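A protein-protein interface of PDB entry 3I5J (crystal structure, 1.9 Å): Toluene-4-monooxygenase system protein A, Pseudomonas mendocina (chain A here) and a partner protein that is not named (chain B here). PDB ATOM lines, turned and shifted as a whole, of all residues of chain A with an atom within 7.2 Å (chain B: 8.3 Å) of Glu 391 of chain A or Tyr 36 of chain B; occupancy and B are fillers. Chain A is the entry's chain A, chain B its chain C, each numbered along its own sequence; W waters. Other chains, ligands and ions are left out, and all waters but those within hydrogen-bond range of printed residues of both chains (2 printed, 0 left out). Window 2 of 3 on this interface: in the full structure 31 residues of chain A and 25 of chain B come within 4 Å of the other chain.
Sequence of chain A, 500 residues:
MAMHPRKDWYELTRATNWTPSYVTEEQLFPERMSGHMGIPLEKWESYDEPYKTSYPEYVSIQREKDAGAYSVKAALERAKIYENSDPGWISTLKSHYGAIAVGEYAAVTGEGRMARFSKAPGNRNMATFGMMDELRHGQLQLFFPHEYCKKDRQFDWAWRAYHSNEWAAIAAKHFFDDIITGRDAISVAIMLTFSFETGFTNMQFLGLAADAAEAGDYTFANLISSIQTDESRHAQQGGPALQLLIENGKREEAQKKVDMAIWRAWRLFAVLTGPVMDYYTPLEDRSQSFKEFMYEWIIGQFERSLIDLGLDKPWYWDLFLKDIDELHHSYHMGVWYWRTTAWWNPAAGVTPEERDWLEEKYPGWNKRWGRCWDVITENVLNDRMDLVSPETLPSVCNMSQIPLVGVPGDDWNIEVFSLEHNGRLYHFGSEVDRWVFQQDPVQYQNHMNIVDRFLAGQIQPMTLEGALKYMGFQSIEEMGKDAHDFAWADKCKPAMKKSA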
ATOM      1  N   TYR A 337     -26.274 -12.761  -6.263  1.00  0.00           N
ATOM      2  CA  TYR A 337     -26.376 -12.269  -4.858  1.00  0.00           C
ATOM      3  C   TYR A 337     -24.995 -11.856  -4.278  1.00  0.00           C
ATOM      4  O   TYR A 337     -24.895 -10.887  -3.538  1.00  0.00           O
ATOM      5  CB  TYR A 337     -27.072 -13.297  -3.940  1.00  0.00           C
ATOM      6  CG  TYR A 337     -27.649 -12.682  -2.662  1.00  0.00           C
ATOM      7  CD1 TYR A 337     -28.910 -12.059  -2.660  1.00  0.00           C
ATOM      8  CD2 TYR A 337     -26.902 -12.659  -1.470  1.00  0.00           C
ATOM      9  CE1 TYR A 337     -29.452 -11.513  -1.497  1.00  0.00           C
ATOM     10  CE2 TYR A 337     -27.451 -12.125  -0.273  1.00  0.00           C
ATOM     11  CZ  TYR A 337     -28.704 -11.528  -0.314  1.00  0.00           C
ATOM     12  OH  TYR A 337     -29.219 -10.954   0.824  1.00  0.00           O
ATOM     13  N   TRP A 338     -23.938 -12.590  -4.666  1.00  0.00           N
ATOM     14  CA  TRP A 338     -22.556 -12.297  -4.272  1.00  0.00           C
ATOM     15  C   TRP A 338     -21.850 -11.500  -5.419  1.00  0.00           C
ATOM     16  O   TRP A 338     -20.637 -11.658  -5.625  1.00  0.00           O
ATOM     17  CB  TRP A 338     -21.819 -13.603  -3.870  1.00  0.00           C
ATOM     18  CG  TRP A 338     -22.084 -14.014  -2.375  1.00  0.00           C
ATOM     19  CD1 TRP A 338     -21.318 -13.684  -1.266  1.00  0.00           C
ATOM     20  CD2 TRP A 338     -23.224 -14.734  -1.869  1.00  0.00           C
ATOM     21  NE1 TRP A 338     -21.889 -14.190  -0.120  1.00  0.00           N
ATOM     22  CE2 TRP A 338     -23.060 -14.832  -0.448  1.00  0.00           C
ATOM     23  CE3 TRP A 338     -24.361 -15.323  -2.476  1.00  0.00           C
ATOM     24  CZ2 TRP A 338     -23.978 -15.483   0.373  1.00  0.00           C
ATOM     25  CZ3 TRP A 338     -25.282 -15.983  -1.645  1.00  0.00           C
ATOM     26  CH2 TRP A 338     -25.080 -16.059  -0.229  1.00  0.00           C
ATOM     27  N   ASP A 386     -29.985  -3.250   1.837  1.00  0.00           N
ATOM     28  CA  ASP A 386     -29.165  -4.136   2.689  1.00  0.00           C
ATOM     29  C   ASP A 386     -29.544  -5.619   2.595  1.00  0.00           C
ATOM     30  O   ASP A 386     -28.723  -6.493   2.862  1.00  0.00           O
ATOM     31  CB  ASP A 386     -29.260  -3.712   4.152  1.00  0.00           C
ATOM     32  CG  ASP A 386     -30.685  -3.595   4.618  1.00  0.00           C
ATOM     33  OD1 ASP A 386     -30.977  -4.120   5.697  1.00  0.00           O
ATOM     34  OD2 ASP A 386     -31.512  -2.973   3.896  1.00  0.00           O
ATOM     35  N   LEU A 387     -30.794  -5.914   2.268  1.00  0.00           N
ATOM     36  CA  LEU A 387     -31.256  -7.298   2.171  1.00  0.00           C
ATOM     37  C   LEU A 387     -30.834  -7.936   0.807  1.00  0.00           C
ATOM     38  O   LEU A 387     -31.155  -9.100   0.513  1.00  0.00           O
ATOM     39  CB  LEU A 387     -32.785  -7.390   2.425  1.00  0.00           C
ATOM     40  CG  LEU A 387     -33.141  -6.772   3.806  1.00  0.00           C
ATOM     41  CD1 LEU A 387     -34.644  -6.821   4.085  1.00  0.00           C
ATOM     42  CD2 LEU A 387     -32.329  -7.472   4.877  1.00  0.00           C
ATOM     43  N   SER A 389     -27.555  -7.534  -0.437  1.00  0.00           N
ATOM     44  CA  SER A 389     -26.131  -7.780  -0.319  1.00  0.00           C
ATOM     45  C   SER A 389     -25.841  -8.758   0.776  1.00  0.00           C
ATOM     46  O   SER A 389     -26.452  -8.677   1.856  1.00  0.00           O
ATOM     47  CB  SER A 389     -25.457  -6.493   0.028  1.00  0.00           C
ATOM     48  OG  SER A 389     -25.244  -5.814  -1.193  1.00  0.00           O
ATOM     49  N   PRO A 390     -24.879  -9.649   0.573  1.00  0.00           N
ATOM     50  CA  PRO A 390     -24.750 -10.664   1.614  1.00  0.00           C
ATOM     51  C   PRO A 390     -23.827 -10.221   2.720  1.00  0.00           C
ATOM     52  O   PRO A 390     -23.020  -9.295   2.534  1.00  0.00           O
ATOM     53  CB  PRO A 390     -24.091 -11.823   0.879  1.00  0.00           C
ATOM     54  CG  PRO A 390     -23.170 -11.055  -0.092  1.00  0.00           C
ATOM     55  CD  PRO A 390     -24.033  -9.949  -0.590  1.00  0.00           C
ATOM     56  N   GLU A 391     -23.935 -10.914   3.845  1.00  0.00           N
ATOM     57  CA  GLU A 391     -23.109 -10.664   5.003  1.00  0.00           C
ATOM     58  C   GLU A 391     -22.468 -11.915   5.479  1.00  0.00           C
ATOM     59  O   GLU A 391     -22.170 -12.038   6.671  1.00  0.00           O
ATOM     60  CB  GLU A 391     -23.976 -10.092   6.151  1.00  0.00           C
ATOM     61  CG  GLU A 391     -24.619  -8.761   5.690  1.00  0.00           C
ATOM     62  CD  GLU A 391     -25.553  -8.134   6.700  1.00  0.00           C
ATOM     63  OE1 GLU A 391     -25.474  -8.453   7.907  1.00  0.00           O
ATOM     64  OE2 GLU A 391     -26.353  -7.279   6.278  1.00  0.00           O
ATOM     65  N   THR A 392     -22.313 -12.913   4.614  1.00  0.00           N
ATOM     66  CA  THR A 392     -21.499 -14.047   4.992  1.00  0.00           C
ATOM     67  C   THR A 392     -20.982 -14.688   3.709  1.00  0.00           C
ATOM     68  O   THR A 392     -21.200 -14.106   2.645  1.00  0.00           O
ATOM     69  CB  THR A 392     -22.275 -15.042   5.788  1.00  0.00           C
ATOM     70  OG1 THR A 392     -21.351 -16.034   6.263  1.00  0.00           O
ATOM     71  CG2 THR A 392     -23.435 -15.721   4.945  1.00  0.00           C
ATOM     72  N   LEU A 393     -20.287 -15.829   3.805  1.00  0.00           N
ATOM     73  CA  LEU A 393     -19.830 -16.534   2.550  1.00  0.00           C
ATOM     74  C   LEU A 393     -20.723 -17.728   2.218  1.00  0.00           C
ATOM     75  O   LEU A 393     -21.301 -18.360   3.119  1.00  0.00           O
ATOM     76  CB  LEU A 393     -18.349 -16.982   2.620  1.00  0.00           C
ATOM     77  CG  LEU A 393     -17.288 -15.852   2.715  1.00  0.00           C
ATOM     78  CD1 LEU A 393     -15.862 -16.432   2.757  1.00  0.00           C
ATOM     79  CD2 LEU A 393     -17.386 -14.799   1.598  1.00  0.00           C
ATOM     80  N   LEU A 464     -15.856  -9.789   4.985  1.00  0.00           N
ATOM     81  CA  LEU A 464     -16.135  -9.816   3.544  1.00  0.00           C
ATOM     82  C   LEU A 464     -15.146  -8.895   2.821  1.00  0.00           C
ATOM     83  O   LEU A 464     -14.599  -9.234   1.734  1.00  0.00           O
ATOM     84  CB  LEU A 464     -17.590  -9.437   3.205  1.00  0.00           C
ATOM     85  CG  LEU A 464     -17.819  -9.002   1.724  1.00  0.00           C
ATOM     86  CD1 LEU A 464     -18.071 -10.208   0.770  1.00  0.00           C
ATOM     87  CD2 LEU A 464     -18.937  -7.881   1.602  1.00  0.00           C
ATOM     88  N   PHE B  10     -30.985 -23.289   4.803  1.00  0.00           N
ATOM     89  CA  PHE B  10     -32.295 -22.887   5.372  1.00  0.00           C
ATOM     90  C   PHE B  10     -33.425 -23.366   4.485  1.00  0.00           C
ATOM     91  O   PHE B  10     -33.313 -23.244   3.243  1.00  0.00           O
ATOM     92  CB  PHE B  10     -32.388 -21.400   5.485  1.00  0.00           C
ATOM     93  CG  PHE B  10     -33.465 -20.924   6.393  1.00  0.00           C
ATOM     94  CD1 PHE B  10     -34.753 -20.776   5.913  1.00  0.00           C
ATOM     95  CD2 PHE B  10     -33.181 -20.652   7.709  1.00  0.00           C
ATOM     96  CE1 PHE B  10     -35.782 -20.289   6.762  1.00  0.00           C
ATOM     97  CE2 PHE B  10     -34.154 -20.164   8.559  1.00  0.00           C
ATOM     98  CZ  PHE B  10     -35.470 -20.021   8.105  1.00  0.00           C
ATOM     99  N   GLN B  17     -24.824 -22.102   3.353  1.00  0.00           N
ATOM    100  CA  GLN B  17     -24.011 -20.958   3.702  1.00  0.00           C
ATOM    101  C   GLN B  17     -23.189 -21.214   4.922  1.00  0.00           C
ATOM    102  O   GLN B  17     -23.662 -21.941   5.848  1.00  0.00           O
ATOM    103  CB  GLN B  17     -24.895 -19.724   4.000  1.00  0.00           C
ATOM    104  CG  GLN B  17     -25.499 -19.046   2.781  1.00  0.00           C
ATOM    105  CD  GLN B  17     -26.417 -17.929   3.214  1.00  0.00           C
ATOM    106  OE1 GLN B  17     -27.232 -18.118   4.148  1.00  0.00           O
ATOM    107  NE2 GLN B  17     -26.293 -16.781   2.617  1.00  0.00           N
ATOM    108  N   LEU B  18     -22.007 -20.593   4.964  1.00  0.00           N
ATOM    109  CA  LEU B  18     -21.207 -20.554   6.179  1.00  0.00           C
ATOM    110  C   LEU B  18     -21.833 -19.635   7.251  1.00  0.00           C
ATOM    111  O   LEU B  18     -21.977 -18.394   7.026  1.00  0.00           O
ATOM    112  CB  LEU B  18     -19.808 -20.057   5.884  1.00  0.00           C
ATOM    113  CG  LEU B  18     -18.996 -19.691   7.150  1.00  0.00           C
ATOM    114  CD1 LEU B  18     -18.555 -20.962   7.944  1.00  0.00           C
ATOM    115  CD2 LEU B  18     -17.784 -18.760   6.845  1.00  0.00           C
ATOM    116  N   VAL B  19     -22.210 -20.191   8.405  1.00  0.00           N
ATOM    117  CA  VAL B  19     -22.708 -19.343   9.499  1.00  0.00           C
ATOM    118  C   VAL B  19     -21.911 -19.641  10.718  1.00  0.00           C
ATOM    119  O   VAL B  19     -21.747 -20.795  11.091  1.00  0.00           O
ATOM    120  CB  VAL B  19     -24.171 -19.579   9.844  1.00  0.00           C
ATOM    121  CG1 VAL B  19     -24.628 -18.663  11.037  1.00  0.00           C
ATOM    122  CG2 VAL B  19     -25.074 -19.393   8.586  1.00  0.00           C
ATOM    123  N   VAL B  20     -21.414 -18.613  11.369  1.00  0.00           N
ATOM    124  CA  VAL B  20     -20.609 -18.868  12.561  1.00  0.00           C
ATOM    125  C   VAL B  20     -21.423 -18.715  13.813  1.00  0.00           C
ATOM    126  O   VAL B  20     -21.737 -17.598  14.203  1.00  0.00           O
ATOM    127  CB  VAL B  20     -19.415 -17.905  12.698  1.00  0.00           C
ATOM    128  CG1 VAL B  20     -18.793 -18.022  14.139  1.00  0.00           C
ATOM    129  CG2 VAL B  20     -18.426 -18.160  11.565  1.00  0.00           C
ATOM    130  N   GLN B  29     -31.190 -20.467  19.145  1.00  0.00           N
ATOM    131  CA  GLN B  29     -30.335 -19.331  18.798  1.00  0.00           C
ATOM    132  C   GLN B  29     -29.594 -19.585  17.488  1.00  0.00           C
ATOM    133  O   GLN B  29     -29.480 -18.675  16.617  1.00  0.00           O
ATOM    134  CB  GLN B  29     -29.358 -19.032  19.938  1.00  0.00           C
ATOM    135  CG  GLN B  29     -30.056 -18.324  21.116  1.00  0.00           C
ATOM    136  CD  GLN B  29     -29.192 -18.250  22.327  1.00  0.00           C
ATOM    137  OE1 GLN B  29     -28.531 -19.225  22.699  1.00  0.00           O
ATOM    138  NE2 GLN B  29     -29.211 -17.093  22.991  1.00  0.00           N
ATOM    139  N   VAL B  30     -29.126 -20.825  17.296  1.00  0.00           N
ATOM    140  CA  VAL B  30     -28.572 -21.168  16.001  1.00  0.00           C
ATOM    141  C   VAL B  30     -29.586 -20.923  14.877  1.00  0.00           C
ATOM    142  O   VAL B  30     -29.191 -20.477  13.773  1.00  0.00           O
ATOM    143  CB  VAL B  30     -28.092 -22.662  15.948  1.00  0.00           C
ATOM    144  CG1 VAL B  30     -27.465 -23.057  14.572  1.00  0.00           C
ATOM    145  CG2 VAL B  30     -27.144 -22.955  17.130  1.00  0.00           C
ATOM    146  N   ALA B  31     -30.861 -21.254  15.086  1.00  0.00           N
ATOM    147  CA  ALA B  31     -31.837 -21.147  13.991  1.00  0.00           C
ATOM    148  C   ALA B  31     -32.099 -19.683  13.626  1.00  0.00           C
ATOM    149  O   ALA B  31     -32.277 -19.347  12.446  1.00  0.00           O
ATOM    150  CB  ALA B  31     -33.139 -21.854  14.329  1.00  0.00           C
ATOM    151  N   GLU B  32     -32.104 -18.819  14.638  1.00  0.00           N
ATOM    152  CA  GLU B  32     -32.087 -17.371  14.436  1.00  0.00           C
ATOM    153  C   GLU B  32     -30.887 -16.880  13.549  1.00  0.00           C
ATOM    154  O   GLU B  32     -31.043 -16.087  12.591  1.00  0.00           O
ATOM    155  CB  GLU B  32     -32.042 -16.658  15.788  1.00  0.00           C
ATOM    156  CG  GLU B  32     -32.649 -15.318  15.698  1.00  0.00           C
ATOM    157  CD  GLU B  32     -34.143 -15.404  15.385  1.00  0.00           C
ATOM    158  OE1 GLU B  32     -34.793 -16.372  15.871  1.00  0.00           O
ATOM    159  OE2 GLU B  32     -34.661 -14.501  14.667  1.00  0.00           O
ATOM    160  N   LYS B  33     -29.694 -17.355  13.886  1.00  0.00           N
ATOM    161  CA  LYS B  33     -28.478 -16.848  13.260  1.00  0.00           C
ATOM    162  C   LYS B  33     -28.392 -17.273  11.794  1.00  0.00           C
ATOM    163  O   LYS B  33     -27.822 -16.589  10.990  1.00  0.00           O
ATOM    164  CB  LYS B  33     -27.225 -17.309  14.014  1.00  0.00           C
ATOM    165  CG  LYS B  33     -27.069 -16.552  15.342  1.00  0.00           C
ATOM    166  CD  LYS B  33     -25.859 -17.047  16.107  1.00  0.00           C
ATOM    167  CE  LYS B  33     -25.648 -16.267  17.450  1.00  0.00           C
ATOM    168  NZ  LYS B  33     -24.385 -16.672  18.119  1.00  0.00           N
ATOM    169  N   VAL B  34     -29.010 -18.380  11.470  1.00  0.00           N
ATOM    170  CA  VAL B  34     -29.029 -18.836  10.104  1.00  0.00           C
ATOM    171  C   VAL B  34     -30.092 -17.992   9.392  1.00  0.00           C
ATOM    172  O   VAL B  34     -29.779 -17.353   8.371  1.00  0.00           O
ATOM    173  CB  VAL B  34     -29.295 -20.336  10.026  1.00  0.00           C
ATOM    174  CG1 VAL B  34     -29.592 -20.763   8.554  1.00  0.00           C
ATOM    175  CG2 VAL B  34     -28.107 -21.078  10.598  1.00  0.00           C
ATOM    176  N   ALA B  35     -31.320 -17.941   9.985  1.00  0.00           N
ATOM    177  CA  ALA B  35     -32.421 -17.136   9.427  1.00  0.00           C
ATOM    178  C   ALA B  35     -32.006 -15.697   9.057  1.00  0.00           C
ATOM    179  O   ALA B  35     -32.461 -15.136   8.046  1.00  0.00           O
ATOM    180  CB  ALA B  35     -33.633 -17.134  10.397  1.00  0.00           C
ATOM    181  N   TYR B  36     -31.097 -15.138   9.866  1.00  0.00           N
ATOM    182  CA  TYR B  36     -30.576 -13.822   9.617  1.00  0.00           C
ATOM    183  C   TYR B  36     -30.051 -13.660   8.173  1.00  0.00           C
ATOM    184  O   TYR B  36     -30.112 -12.574   7.578  1.00  0.00           O
ATOM    185  CB  TYR B  36     -29.433 -13.496  10.563  1.00  0.00           C
ATOM    186  CG  TYR B  36     -28.929 -12.105  10.261  1.00  0.00           C
ATOM    187  CD1 TYR B  36     -29.472 -10.994  10.925  1.00  0.00           C
ATOM    188  CD2 TYR B  36     -27.986 -11.878   9.240  1.00  0.00           C
ATOM    189  CE1 TYR B  36     -29.035  -9.663  10.642  1.00  0.00           C
ATOM    190  CE2 TYR B  36     -27.536 -10.564   8.943  1.00  0.00           C
ATOM    191  CZ  TYR B  36     -28.068  -9.460   9.625  1.00  0.00           C
ATOM    192  OH  TYR B  36     -27.644  -8.152   9.340  1.00  0.00           O
ATOM    193  N   HIS B  37     -29.493 -14.732   7.638  1.00  0.00           N
ATOM    194  CA  HIS B  37     -28.820 -14.621   6.380  1.00  0.00           C
ATOM    195  C   HIS B  37     -29.740 -15.135   5.271  1.00  0.00           C
ATOM    196  O   HIS B  37     -29.294 -15.376   4.149  1.00  0.00           O
ATOM    197  CB  HIS B  37     -27.496 -15.382   6.449  1.00  0.00           C
ATOM    198  CG  HIS B  37     -26.470 -14.770   7.363  1.00  0.00           C
ATOM    199  ND1 HIS B  37     -25.695 -13.692   7.003  1.00  0.00           N
ATOM    200  CD2 HIS B  37     -26.080 -15.101   8.620  1.00  0.00           C
ATOM    201  CE1 HIS B  37     -24.863 -13.397   7.985  1.00  0.00           C
ATOM    202  NE2 HIS B  37     -25.071 -14.244   8.975  1.00  0.00           N
ATOM    203  N   CYS B  38     -31.033 -15.251   5.551  1.00  0.00           N
ATOM    204  CA  CYS B  38     -31.939 -15.984   4.657  1.00  0.00           C
ATOM    205  C   CYS B  38     -33.333 -15.400   4.552  1.00  0.00           C
ATOM    206  O   CYS B  38     -33.846 -15.126   3.460  1.00  0.00           O
ATOM    207  CB  CYS B  38     -32.110 -17.429   5.137  1.00  0.00           C
ATOM    208  SG  CYS B  38     -30.620 -18.399   5.120  1.00  0.00           S
ATOM    209  N   VAL B  39     -33.992 -15.342   5.707  1.00  0.00           N
ATOM    210  CA  VAL B  39     -35.358 -14.932   5.740  1.00  0.00           C
ATOM    211  C   VAL B  39     -35.387 -13.445   5.383  1.00  0.00           C
ATOM    212  O   VAL B  39     -34.603 -12.643   5.875  1.00  0.00           O
ATOM    213  CB  VAL B  39     -36.028 -15.271   7.131  1.00  0.00           C
ATOM    214  CG1 VAL B  39     -37.268 -14.525   7.327  1.00  0.00           C
ATOM    215  CG2 VAL B  39     -36.258 -16.811   7.219  1.00  0.00           C
ATOM    216  N   ASN B  40     -36.247 -13.131   4.417  1.00  0.00           N
ATOM    217  CA  ASN B  40     -36.448 -11.733   3.933  1.00  0.00           C
ATOM    218  C   ASN B  40     -35.290 -11.295   3.024  1.00  0.00           C
ATOM    219  O   ASN B  40     -35.160 -10.116   2.726  1.00  0.00           O
ATOM    220  CB  ASN B  40     -36.644 -10.734   5.067  1.00  0.00           C
ATOM    221  CG  ASN B  40     -38.066 -10.743   5.621  1.00  0.00           C
ATOM    222  OD1 ASN B  40     -39.047 -10.754   4.858  1.00  0.00           O
ATOM    223  ND2 ASN B  40     -38.190 -10.743   6.936  1.00  0.00           N
ATOM    224  N   ARG B  41     -34.435 -12.251   2.651  1.00  0.00           N
ATOM    225  CA  ARG B  41     -33.409 -12.039   1.664  1.00  0.00           C
ATOM    226  C   ARG B  41     -33.759 -12.878   0.479  1.00  0.00           C
ATOM    227  O   ARG B  41     -33.926 -12.339  -0.628  1.00  0.00           O
ATOM    228  CB  ARG B  41     -32.021 -12.459   2.154  1.00  0.00           C
ATOM    229  CG  ARG B  41     -31.528 -11.497   3.265  1.00  0.00           C
ATOM    230  CD  ARG B  41     -30.175 -11.889   3.711  1.00  0.00           C
ATOM    231  NE  ARG B  41     -29.748 -11.046   4.832  1.00  0.00           N
ATOM    232  CZ  ARG B  41     -28.945 -10.011   4.706  1.00  0.00           C
ATOM    233  NH1 ARG B  41     -28.449  -9.700   3.515  1.00  0.00           N
ATOM    234  NH2 ARG B  41     -28.578  -9.344   5.769  1.00  0.00           N
ATOM    235  N   ARG B  42     -33.846 -14.204   0.715  1.00  0.00           N
ATOM    236  CA  ARG B  42     -34.216 -15.085  -0.415  1.00  0.00           C
ATOM    237  C   ARG B  42     -35.399 -15.985  -0.090  1.00  0.00           C
ATOM    238  O   ARG B  42     -35.904 -16.666  -0.996  1.00  0.00           O
ATOM    239  CB  ARG B  42     -32.981 -15.896  -0.894  1.00  0.00           C
ATOM    240  CG  ARG B  42     -31.844 -14.971  -1.409  1.00  0.00           C
ATOM    241  CD  ARG B  42     -30.638 -15.846  -1.813  1.00  0.00           C
ATOM    242  NE  ARG B  42     -30.349 -16.623  -0.636  1.00  0.00           N
ATOM    243  CZ  ARG B  42     -29.679 -16.127   0.399  1.00  0.00           C
ATOM    244  NH1 ARG B  42     -29.521 -16.858   1.481  1.00  0.00           N
ATOM    245  NH2 ARG B  42     -29.180 -14.910   0.336  1.00  0.00           N
ATOM    246  N   MET B  50     -38.889 -22.747  14.086  1.00  0.00           N
ATOM    247  CA  MET B  50     -37.728 -23.246  13.328  1.00  0.00           C
ATOM    248  C   MET B  50     -36.995 -24.281  14.172  1.00  0.00           C
ATOM    249  O   MET B  50     -36.904 -24.122  15.376  1.00  0.00           O
ATOM    250  CB  MET B  50     -36.790 -22.125  12.920  1.00  0.00           C
ATOM    251  CG  MET B  50     -37.442 -20.901  12.250  1.00  0.00           C
ATOM    252  SD  MET B  50     -36.117 -19.728  11.722  1.00  0.00           S
ATOM    253  CE  MET B  50     -35.757 -18.815  13.269  1.00  0.00           C
HETATM  254  O   HOH W   1     -26.224 -12.426   4.478  1.00  0.00           O
HETATM  255  O   HOH W   2     -33.574  -9.624  -1.302  1.00  0.00           O
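The side-chain hydroxyl (OH) of Tyr 337 of chain A sits at hydrogen-bond distance from the guanidinium group (NH1) of Arg 41 of chain B (3.1 Å).
O of Asp 386 of chain A is in hydrogen-bond range of NH1 of Arg 41 of chain B (3.3 Å).
O of Ser 389 of chain A is in hydrogen-bond range of NH1 of Arg 41 of chain B.
OE1 of Glu 391 of chain A sits at hydrogen-bond distance from OH of Tyr 36 of chain B (2.6 Å).
OE2 of Glu 391 of chain A is in salt-bridge range of NH2 of Arg 41 of chain B (3.1 Å).
The side-chain hydroxyl (OG1) of Thr 392 of chain A sits at hydrogen-bond distance from the backbone carbonyl oxygen (O) of Leu 18 of chain B, at 2.6 Å.
The backbone NH of Leu 18 of chain B is in hydrogen-bond range of the backbone carbonyl oxygen of Leu 393 of chain A (3.0 Å).
Water W1 bridges N of Glu 391 of chain A (2.8 Å) and ND1 of His 37 of chain B (2.9 Å).
Water W2 bridges O of Arg 41 of chain B and O of Leu 387 of chain A.
The backbone carbonyl oxygen (O) of Thr 392 of chain A sits at hydrogen-bond distance from the indole nitrogen (NE1) of Trp 338 of chain A (2.9 Å).
OE1 of Gln 17 of chain B lies close to O of His 37 of chain B (3.4 Å).
The side-chain amide oxygen of Gln 17 of chain B is in hydrogen-bond range of the side-chain sulfur of Cys 38 of chain B (3.5 Å).
The side-chain amide nitrogen of Gln 17 of chain B sits close to the guanidinium group of Arg 42 of chain B (3.4 Å).
The backbone carbonyl oxygen of Tyr 36 of chain B lies within hydrogen-bond range of the guanidinium group of Arg 41 of chain B, 3.2 Å away.
O of His 37 of chain B sits at hydrogen-bond distance from NH1 of Arg 42 of chain B.
Among the printed residues, merely in contact across the chains: Tyr 337 of chain A with Arg 42 of chain B (3.3 Å), Trp 338 of chain A with Gln 17 of chain B (3.2 Å), Leu 387 of chain A with Asn 40 of chain B (3.6 Å), Leu 387 of chain A with Arg 41 of chain B (3.7 Å), Glu 391 of chain A with His 37 of chain B (3.3 Å), Thr 392 of chain A with Gln 17 of chain B (3.8 Å), Thr 392 of chain A with His 37 of chain B (3.7 Å) and Leu 393 of chain A with Gln 17 of chain B (3.8 Å).
Hydrophobic or aromatic side chains of chain A within 4 Å of the printed part of chain B: Tyr 337, Trp 338 and Leu 387.
Among the printed residues, 15 pairs touch across the chains.
Printed residues of chain B within 4 Å of Trp 338 of chain A: Gln 17.
Printed residues of chain B within 4 Å of Leu 387 of chain A: Asn 40 (3.6 Å) and Arg 41 (3.7 Å).
Pro 390 of chain A touches none of the printed residues of chain B.
Tyr 36 of chain B touches one residue of chain A.
Met 50 of chain B touches none of the printed residues of chain A.
The nearest residue of chain B that does not touch Glu 391 of chain A is Leu 18 of chain B (6.4 Å).
The nearest printed residue of chain B that does not touch Leu 387 of chain A is Val 39 of chain B (5.7 Å).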
